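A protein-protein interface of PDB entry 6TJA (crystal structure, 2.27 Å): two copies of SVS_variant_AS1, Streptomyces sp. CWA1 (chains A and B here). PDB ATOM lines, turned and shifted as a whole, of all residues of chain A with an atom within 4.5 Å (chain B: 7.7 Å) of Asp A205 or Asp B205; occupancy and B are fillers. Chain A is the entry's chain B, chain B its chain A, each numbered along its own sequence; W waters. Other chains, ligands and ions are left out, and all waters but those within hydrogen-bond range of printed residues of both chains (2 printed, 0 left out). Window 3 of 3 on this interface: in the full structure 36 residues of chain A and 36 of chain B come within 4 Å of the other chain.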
ATOM      1  N   THR A 144       7.759 -14.194  -1.461  1.00  0.00           N
ATOM      2  CA  THR A 144       8.339 -15.551  -1.473  1.00  0.00           C
ATOM      3  C   THR A 144       7.225 -16.603  -1.535  1.00  0.00           C
ATOM      4  O   THR A 144       7.314 -17.469  -2.402  1.00  0.00           O
ATOM      5  CB  THR A 144       9.284 -15.795  -0.286  1.00  0.00           C
ATOM      6  OG1 THR A 144      10.447 -14.987  -0.457  1.00  0.00           O
ATOM      7  CG2 THR A 144       9.742 -17.234  -0.205  1.00  0.00           C
ATOM      8  N   ARG A 148       6.233 -19.328  -4.589  1.00  0.00           N
ATOM      9  CA  ARG A 148       6.065 -20.796  -4.422  1.00  0.00           C
ATOM     10  C   ARG A 148       4.710 -21.212  -5.026  1.00  0.00           C
ATOM     11  O   ARG A 148       4.683 -22.152  -5.770  1.00  0.00           O
ATOM     12  CB  ARG A 148       6.197 -21.179  -2.947  1.00  0.00           C
ATOM     13  CG  ARG A 148       7.588 -20.921  -2.380  1.00  0.00           C
ATOM     14  CD  ARG A 148       7.664 -21.176  -0.881  1.00  0.00           C
ATOM     15  NE  ARG A 148       9.018 -20.981  -0.407  1.00  0.00           N
ATOM     16  CZ  ARG A 148       9.381 -20.996   0.877  1.00  0.00           C
ATOM     17  NH1 ARG A 148       8.473 -21.271   1.811  1.00  0.00           N
ATOM     18  NH2 ARG A 148      10.656 -20.779   1.215  1.00  0.00           N
ATOM     19  N   VAL A 203       7.908 -20.716   5.771  1.00  0.00           N
ATOM     20  CA  VAL A 203       8.974 -21.754   5.852  1.00  0.00           C
ATOM     21  C   VAL A 203      10.212 -21.212   5.160  1.00  0.00           C
ATOM     22  O   VAL A 203      10.169 -20.906   3.976  1.00  0.00           O
ATOM     23  CB  VAL A 203       8.545 -23.085   5.223  1.00  0.00           C
ATOM     24  CG1 VAL A 203       9.605 -24.153   5.443  1.00  0.00           C
ATOM     25  CG2 VAL A 203       7.184 -23.534   5.730  1.00  0.00           C
ATOM     26  N   PRO A 204      11.357 -21.108   5.857  1.00  0.00           N
ATOM     27  CA  PRO A 204      12.561 -20.562   5.243  1.00  0.00           C
ATOM     28  C   PRO A 204      12.956 -21.478   4.069  1.00  0.00           C
ATOM     29  O   PRO A 204      12.747 -22.702   4.197  1.00  0.00           O
ATOM     30  CB  PRO A 204      13.609 -20.555   6.383  1.00  0.00           C
ATOM     31  CG  PRO A 204      12.822 -20.794   7.655  1.00  0.00           C
ATOM     32  CD  PRO A 204      11.582 -21.557   7.241  1.00  0.00           C
ATOM     33  N   ASP A 205      13.464 -20.889   2.975  1.00  0.00           N
ATOM     34  CA  ASP A 205      14.041 -21.574   1.778  1.00  0.00           C
ATOM     35  C   ASP A 205      14.871 -22.816   2.184  1.00  0.00           C
ATOM     36  O   ASP A 205      14.648 -23.917   1.625  1.00  0.00           O
ATOM     37  CB  ASP A 205      14.889 -20.604   0.938  1.00  0.00           C
ATOM     38  CG  ASP A 205      15.657 -19.520   1.696  1.00  0.00           C
ATOM     39  OD1 ASP A 205      15.945 -19.714   2.922  1.00  0.00           O
ATOM     40  OD2 ASP A 205      15.977 -18.458   1.060  1.00  0.00           O
ATOM     41  N   ARG A 206      15.809 -22.644   3.113  1.00  0.00           N
ATOM     42  CA  ARG A 206      16.820 -23.645   3.514  1.00  0.00           C
ATOM     43  C   ARG A 206      16.090 -24.912   3.966  1.00  0.00           C
ATOM     44  O   ARG A 206      16.590 -26.005   3.685  1.00  0.00           O
ATOM     45  CB  ARG A 206      17.704 -23.008   4.589  1.00  0.00           C
ATOM     46  CG  ARG A 206      18.815 -23.877   5.164  1.00  0.00           C
ATOM     47  CD  ARG A 206      19.188 -23.375   6.560  1.00  0.00           C
ATOM     48  NE  ARG A 206      18.761 -21.982   6.766  1.00  0.00           N
ATOM     49  CZ  ARG A 206      17.718 -21.563   7.506  1.00  0.00           C
ATOM     50  NH1 ARG A 206      16.954 -22.416   8.174  1.00  0.00           N
ATOM     51  NH2 ARG A 206      17.449 -20.268   7.575  1.00  0.00           N
ATOM     52  N   GLU A 207      14.918 -24.774   4.578  1.00  0.00           N
ATOM     53  CA  GLU A 207      14.114 -25.933   5.032  1.00  0.00           C
ATOM     54  C   GLU A 207      13.140 -26.352   3.929  1.00  0.00           C
ATOM     55  O   GLU A 207      13.028 -27.574   3.673  1.00  0.00           O
ATOM     56  CB  GLU A 207      13.455 -25.626   6.376  1.00  0.00           C
ATOM     57  CG  GLU A 207      14.404 -25.851   7.562  1.00  0.00           C
ATOM     58  CD  GLU A 207      13.755 -25.647   8.932  1.00  0.00           C
ATOM     59  OE1 GLU A 207      13.380 -24.474   9.221  1.00  0.00           O
ATOM     60  OE2 GLU A 207      13.596 -26.667   9.707  1.00  0.00           O
ATOM     61  N   MET A 208      12.452 -25.409   3.287  1.00  0.00           N
ATOM     62  CA  MET A 208      11.420 -25.773   2.274  1.00  0.00           C
ATOM     63  C   MET A 208      12.037 -26.608   1.141  1.00  0.00           C
ATOM     64  O   MET A 208      11.458 -27.591   0.792  1.00  0.00           O
ATOM     65  CB  MET A 208      10.707 -24.559   1.676  1.00  0.00           C
ATOM     66  CG  MET A 208       9.585 -24.986   0.718  1.00  0.00           C
ATOM     67  SD  MET A 208       8.367 -26.099   1.527  1.00  0.00           S
ATOM     68  CE  MET A 208       7.200 -24.900   2.150  1.00  0.00           C
ATOM     69  N   HIS A 209      13.193 -26.245   0.609  1.00  0.00           N
ATOM     70  CA  HIS A 209      13.792 -26.869  -0.595  1.00  0.00           C
ATOM     71  C   HIS A 209      14.771 -28.005  -0.257  1.00  0.00           C
ATOM     72  O   HIS A 209      15.339 -28.577  -1.203  1.00  0.00           O
ATOM     73  CB  HIS A 209      14.440 -25.770  -1.428  1.00  0.00           C
ATOM     74  CG  HIS A 209      13.459 -24.717  -1.816  1.00  0.00           C
ATOM     75  ND1 HIS A 209      12.241 -25.034  -2.430  1.00  0.00           N
ATOM     76  CD2 HIS A 209      13.498 -23.360  -1.680  1.00  0.00           C
ATOM     77  CE1 HIS A 209      11.569 -23.909  -2.661  1.00  0.00           C
ATOM     78  NE2 HIS A 209      12.331 -22.853  -2.204  1.00  0.00           N
ATOM     79  N   THR B 142      23.041 -24.369  -3.971  1.00  0.00           N
ATOM     80  CA  THR B 142      22.103 -24.780  -2.891  1.00  0.00           C
ATOM     81  C   THR B 142      20.817 -25.375  -3.495  1.00  0.00           C
ATOM     82  O   THR B 142      20.426 -25.086  -4.634  1.00  0.00           O
ATOM     83  CB  THR B 142      21.832 -23.629  -1.919  1.00  0.00           C
ATOM     84  OG1 THR B 142      21.009 -22.703  -2.640  1.00  0.00           O
ATOM     85  CG2 THR B 142      23.118 -23.005  -1.396  1.00  0.00           C
ATOM     86  N   PRO B 143      20.144 -26.287  -2.758  1.00  0.00           N
ATOM     87  CA  PRO B 143      18.819 -26.756  -3.151  1.00  0.00           C
ATOM     88  C   PRO B 143      17.898 -25.582  -3.549  1.00  0.00           C
ATOM     89  O   PRO B 143      17.150 -25.731  -4.497  1.00  0.00           O
ATOM     90  CB  PRO B 143      18.343 -27.528  -1.894  1.00  0.00           C
ATOM     91  CG  PRO B 143      19.660 -28.024  -1.216  1.00  0.00           C
ATOM     92  CD  PRO B 143      20.627 -26.891  -1.487  1.00  0.00           C
ATOM     93  N   THR B 144      17.986 -24.444  -2.853  1.00  0.00           N
ATOM     94  CA  THR B 144      17.196 -23.227  -3.174  1.00  0.00           C
ATOM     95  C   THR B 144      17.523 -22.763  -4.595  1.00  0.00           C
ATOM     96  O   THR B 144      16.596 -22.525  -5.372  1.00  0.00           O
ATOM     97  CB  THR B 144      17.446 -22.107  -2.156  1.00  0.00           C
ATOM     98  OG1 THR B 144      16.953 -22.553  -0.894  1.00  0.00           O
ATOM     99  CG2 THR B 144      16.734 -20.828  -2.534  1.00  0.00           C
ATOM    100  N   GLN B 145      18.801 -22.657  -4.939  1.00  0.00           N
ATOM    101  CA  GLN B 145      19.200 -22.132  -6.269  1.00  0.00           C
ATOM    102  C   GLN B 145      18.794 -23.141  -7.344  1.00  0.00           C
ATOM    103  O   GLN B 145      18.315 -22.701  -8.403  1.00  0.00           O
ATOM    104  CB  GLN B 145      20.694 -21.860  -6.340  1.00  0.00           C
ATOM    105  CG  GLN B 145      21.146 -20.725  -5.439  1.00  0.00           C
ATOM    106  CD  GLN B 145      22.656 -20.707  -5.372  1.00  0.00           C
ATOM    107  OE1 GLN B 145      23.289 -21.734  -5.094  1.00  0.00           O
ATOM    108  NE2 GLN B 145      23.235 -19.555  -5.683  1.00  0.00           N
ATOM    109  N   ARG B 147      16.216 -25.111  -7.236  1.00  0.00           N
ATOM    110  CA  ARG B 147      14.754 -25.016  -7.443  1.00  0.00           C
ATOM    111  C   ARG B 147      14.446 -23.769  -8.267  1.00  0.00           C
ATOM    112  O   ARG B 147      13.545 -23.836  -9.100  1.00  0.00           O
ATOM    113  CB  ARG B 147      13.983 -24.996  -6.128  1.00  0.00           C
ATOM    114  CG  ARG B 147      13.908 -26.347  -5.432  1.00  0.00           C
ATOM    115  CD  ARG B 147      13.324 -27.494  -6.243  1.00  0.00           C
ATOM    116  NE  ARG B 147      11.887 -27.419  -6.446  1.00  0.00           N
ATOM    117  CZ  ARG B 147      11.204 -28.238  -7.246  1.00  0.00           C
ATOM    118  NH1 ARG B 147      11.842 -29.169  -7.935  1.00  0.00           N
ATOM    119  NH2 ARG B 147       9.888 -28.122  -7.344  1.00  0.00           N
ATOM    120  N   ARG B 148      15.159 -22.674  -8.037  1.00  0.00           N
ATOM    121  CA  ARG B 148      14.990 -21.446  -8.842  1.00  0.00           C
ATOM    122  C   ARG B 148      15.238 -21.820 -10.306  1.00  0.00           C
ATOM    123  O   ARG B 148      14.430 -21.380 -11.144  1.00  0.00           O
ATOM    124  CB  ARG B 148      15.892 -20.319  -8.331  1.00  0.00           C
ATOM    125  CG  ARG B 148      15.506 -19.799  -6.951  1.00  0.00           C
ATOM    126  CD  ARG B 148      16.490 -18.771  -6.415  1.00  0.00           C
ATOM    127  NE  ARG B 148      16.139 -18.302  -5.085  1.00  0.00           N
ATOM    128  CZ  ARG B 148      16.810 -17.382  -4.377  1.00  0.00           C
ATOM    129  NH1 ARG B 148      17.874 -16.772  -4.875  1.00  0.00           N
ATOM    130  NH2 ARG B 148      16.382 -17.039  -3.179  1.00  0.00           N
ATOM    131  N   GLU B 196      23.405 -16.911 -10.434  1.00  0.00           N
ATOM    132  CA  GLU B 196      23.683 -17.241  -9.070  1.00  0.00           C
ATOM    133  C   GLU B 196      24.546 -18.468  -8.938  1.00  0.00           C
ATOM    134  O   GLU B 196      25.368 -18.560  -8.090  1.00  0.00           O
ATOM    135  CB  GLU B 196      22.359 -17.602  -8.452  1.00  0.00           C
ATOM    136  CG  GLU B 196      21.848 -16.638  -7.473  1.00  0.00           C
ATOM    137  CD  GLU B 196      20.830 -17.261  -6.606  1.00  0.00           C
ATOM    138  OE1 GLU B 196      19.735 -17.510  -7.052  1.00  0.00           O
ATOM    139  OE2 GLU B 196      21.137 -17.475  -5.461  1.00  0.00           O
ATOM    140  N   GLU B 202      24.636 -16.529  -3.447  1.00  0.00           N
ATOM    141  CA  GLU B 202      23.214 -16.894  -3.138  1.00  0.00           C
ATOM    142  C   GLU B 202      22.370 -15.664  -2.729  1.00  0.00           C
ATOM    143  O   GLU B 202      22.559 -15.122  -1.610  1.00  0.00           O
ATOM    144  CB  GLU B 202      23.089 -17.970  -2.059  1.00  0.00           C
ATOM    145  CG  GLU B 202      21.653 -18.528  -1.992  1.00  0.00           C
ATOM    146  CD  GLU B 202      21.295 -19.553  -0.911  1.00  0.00           C
ATOM    147  OE1 GLU B 202      22.040 -19.654   0.129  1.00  0.00           O
ATOM    148  OE2 GLU B 202      20.270 -20.262  -1.102  1.00  0.00           O
ATOM    149  N   VAL B 203      21.388 -15.271  -3.550  1.00  0.00           N
ATOM    150  CA  VAL B 203      20.494 -14.111  -3.231  1.00  0.00           C
ATOM    151  C   VAL B 203      19.417 -14.596  -2.263  1.00  0.00           C
ATOM    152  O   VAL B 203      18.716 -15.549  -2.575  1.00  0.00           O
ATOM    153  CB  VAL B 203      19.868 -13.518  -4.502  1.00  0.00           C
ATOM    154  CG1 VAL B 203      19.066 -12.254  -4.231  1.00  0.00           C
ATOM    155  CG2 VAL B 203      20.912 -13.298  -5.573  1.00  0.00           C
ATOM    156  N   PRO B 204      19.250 -13.960  -1.123  1.00  0.00           N
ATOM    157  CA  PRO B 204      18.205 -14.383  -0.203  1.00  0.00           C
ATOM    158  C   PRO B 204      16.804 -14.247  -0.798  1.00  0.00           C
ATOM    159  O   PRO B 204      16.567 -13.356  -1.539  1.00  0.00           O
ATOM    160  CB  PRO B 204      18.388 -13.452   0.975  1.00  0.00           C
ATOM    161  CG  PRO B 204      19.725 -12.907   0.838  1.00  0.00           C
ATOM    162  CD  PRO B 204      20.024 -12.850  -0.597  1.00  0.00           C
ATOM    163  N   ASP B 205      15.911 -15.156  -0.476  1.00  0.00           N
ATOM    164  CA  ASP B 205      14.522 -15.146  -0.958  1.00  0.00           C
ATOM    165  C   ASP B 205      13.854 -13.764  -0.893  1.00  0.00           C
ATOM    166  O   ASP B 205      13.283 -13.330  -1.827  1.00  0.00           O
ATOM    167  CB  ASP B 205      13.658 -16.123  -0.158  1.00  0.00           C
ATOM    168  CG  ASP B 205      13.459 -17.496  -0.823  1.00  0.00           C
ATOM    169  OD1 ASP B 205      14.188 -17.928  -1.704  1.00  0.00           O
ATOM    170  OD2 ASP B 205      12.568 -18.223  -0.405  1.00  0.00           O
ATOM    171  N   ARG B 206      13.950 -13.102   0.238  1.00  0.00           N
ATOM    172  CA  ARG B 206      13.357 -11.821   0.446  1.00  0.00           C
ATOM    173  C   ARG B 206      13.846 -10.757  -0.516  1.00  0.00           C
ATOM    174  O   ARG B 206      13.158  -9.843  -0.801  1.00  0.00           O
ATOM    175  CB  ARG B 206      13.456 -11.399   1.924  1.00  0.00           C
ATOM    176  CG  ARG B 206      14.586 -10.470   2.263  1.00  0.00           C
ATOM    177  CD  ARG B 206      15.275 -10.757   3.583  1.00  0.00           C
ATOM    178  NE  ARG B 206      16.727 -10.785   3.411  1.00  0.00           N
ATOM    179  CZ  ARG B 206      17.478  -9.717   3.159  1.00  0.00           C
ATOM    180  NH1 ARG B 206      16.935  -8.516   3.082  1.00  0.00           N
ATOM    181  NH2 ARG B 206      18.775  -9.853   2.984  1.00  0.00           N
ATOM    182  N   GLU B 207      15.023 -10.930  -1.047  1.00  0.00           N
ATOM    183  CA  GLU B 207      15.584  -9.981  -2.039  1.00  0.00           C
ATOM    184  C   GLU B 207      15.225 -10.504  -3.421  1.00  0.00           C
ATOM    185  O   GLU B 207      14.807  -9.720  -4.248  1.00  0.00           O
ATOM    186  CB  GLU B 207      17.090  -9.792  -1.860  1.00  0.00           C
ATOM    187  CG  GLU B 207      17.468  -8.834  -0.735  1.00  0.00           C
ATOM    188  CD  GLU B 207      18.939  -8.417  -0.746  1.00  0.00           C
ATOM    189  OE1 GLU B 207      19.260  -7.179  -0.941  1.00  0.00           O
ATOM    190  OE2 GLU B 207      19.772  -9.336  -0.567  1.00  0.00           O
ATOM    191  N   MET B 208      15.408 -11.775  -3.665  1.00  0.00           N
ATOM    192  CA  MET B 208      15.128 -12.328  -4.958  1.00  0.00           C
ATOM    193  C   MET B 208      13.692 -12.194  -5.393  1.00  0.00           C
ATOM    194  O   MET B 208      13.457 -11.902  -6.512  1.00  0.00           O
ATOM    195  CB  MET B 208      15.544 -13.788  -5.049  1.00  0.00           C
ATOM    196  CG  MET B 208      15.523 -14.361  -6.454  1.00  0.00           C
ATOM    197  SD  MET B 208      16.356 -13.470  -7.770  1.00  0.00           S
ATOM    198  CE  MET B 208      17.733 -14.509  -8.100  1.00  0.00           C
ATOM    199  N   HIS B 209      12.762 -12.386  -4.474  1.00  0.00           N
ATOM    200  CA  HIS B 209      11.344 -12.342  -4.778  1.00  0.00           C
ATOM    201  C   HIS B 209      10.611 -11.003  -4.727  1.00  0.00           C
ATOM    202  O   HIS B 209       9.468 -10.951  -4.974  1.00  0.00           O
ATOM    203  CB  HIS B 209      10.610 -13.473  -4.077  1.00  0.00           C
ATOM    204  CG  HIS B 209      11.192 -14.812  -4.362  1.00  0.00           C
ATOM    205  ND1 HIS B 209      11.401 -15.272  -5.634  1.00  0.00           N
ATOM    206  CD2 HIS B 209      11.634 -15.780  -3.541  1.00  0.00           C
ATOM    207  CE1 HIS B 209      11.922 -16.473  -5.584  1.00  0.00           C
ATOM    208  NE2 HIS B 209      12.082 -16.800  -4.324  1.00  0.00           N
ATOM    209  N   ARG B 210      11.312  -9.973  -4.311  1.00  0.00           N
ATOM    210  CA  ARG B 210      10.872  -8.559  -4.395  1.00  0.00           C
ATOM    211  C   ARG B 210      10.288  -8.298  -5.784  1.00  0.00           C
ATOM    212  O   ARG B 210      10.952  -8.532  -6.806  1.00  0.00           O
ATOM    213  CB  ARG B 210      12.024  -7.579  -4.140  1.00  0.00           C
ATOM    214  CG  ARG B 210      12.379  -7.345  -2.681  1.00  0.00           C
ATOM    215  CD  ARG B 210      13.597  -6.438  -2.580  1.00  0.00           C
ATOM    216  NE  ARG B 210      13.241  -5.106  -3.020  1.00  0.00           N
ATOM    217  CZ  ARG B 210      14.081  -4.088  -3.226  1.00  0.00           C
ATOM    218  NH1 ARG B 210      15.379  -4.254  -3.080  1.00  0.00           N
ATOM    219  NH2 ARG B 210      13.598  -2.916  -3.618  1.00  0.00           N
HETATM  220  O   HOH W   1      11.319 -20.274  -2.205  1.00  0.00           O
HETATM  221  O   HOH W   2       9.890 -18.753  -3.784  1.00  0.00           O
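NH2 of Arg A148 is in salt-bridge range of OD2 of Asp B205 (3.6 Å).
OD2 of Asp A205 sits close to OD1 of Asp B205, at 3.3 Å.
The guanidinium group of Arg A148 is in hydrogen-bond range of the backbone carbonyl oxygen of Val A203 (2.8 Å).
The side-chain carboxylate of Asp B205 is in salt-bridge range of the guanidinium group of Arg B148, at 2.8 Å.
The side-chain hydroxyl (OG1) of Thr B142 lies close to the backbone NH (N) of Thr B144 (3.5 Å).
Among the printed residues, pairs that only touch across the chains: Thr A144 with Asp B205 (3.0 Å), Thr A144 with His B209 (3.4 Å), Asp A205 with Thr B144 (3.4 Å), His A209 with Pro B143 (3.3 Å), His A209 with Thr B144 (3.6 Å) and His A209 with Arg B147 (3.7 Å).
Asp A205 touches just these residues of chain B: Thr B144 and Asp B205.
Asp B205 touches just these residues of chain A: Thr A144 (3.0 Å), Arg A148 (3.6 Å) and Asp A205 (3.3 Å).
Of the printed residues of chain B, Arg A148 touches Asp B205 (3.6 Å).
Printed residues of chain A within 4 Å of Pro B143: His A209 (3.3 Å).
Of the printed residues of chain A, Thr B144 touches Asp A205 (3.4 Å) and His A209 (3.6 Å).
The nearest residue of chain B that does not touch Asp A205 is Arg B148 (4.5 Å).
The nearest printed residue of chain A that does not touch Asp B205 is His A209 (5.0 Å).
Of the 9 printed residues of chain A, 4 touch a printed residue of chain B.
Hydrophobic or aromatic side chains of chain A within 4 Å of the printed part of chain B: His A209.
Along chain A the printed residues that touch a printed residue of chain B span positions 144 to 209.
Hydrophobic or aromatic side chains of chain B within 4 Å of the printed part of chain A: Pro B143 and His B209.
Among the printed residues, 8 pairs touch across the chains.
Thr A144 touches Asp B205, and with the chains exchanged Asp A205 touches Thr B144.
Thr A144 touches His B209, and with the chains exchanged His A209 touches Thr B144.
Arg A148 touches Asp B205, but with the chains exchanged Asp A205 does not touch Arg B148 (4.5 Å).
Asp A205 touches its own counterpart, Asp B205.
9 positions are printed for both chains.
Water W1 lies within hydrogen-bond range of a ring nitrogen (NE2) of His A209 (2.8 Å), the side-chain carboxylate of Asp B205 (3.0 Å) and the guanidinium group of Arg A148 (3.0 Å).
Water W2 lies within hydrogen-bond range of NE2 of His B209 (3.0 Å) and O of Thr A144 (3.2 Å).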
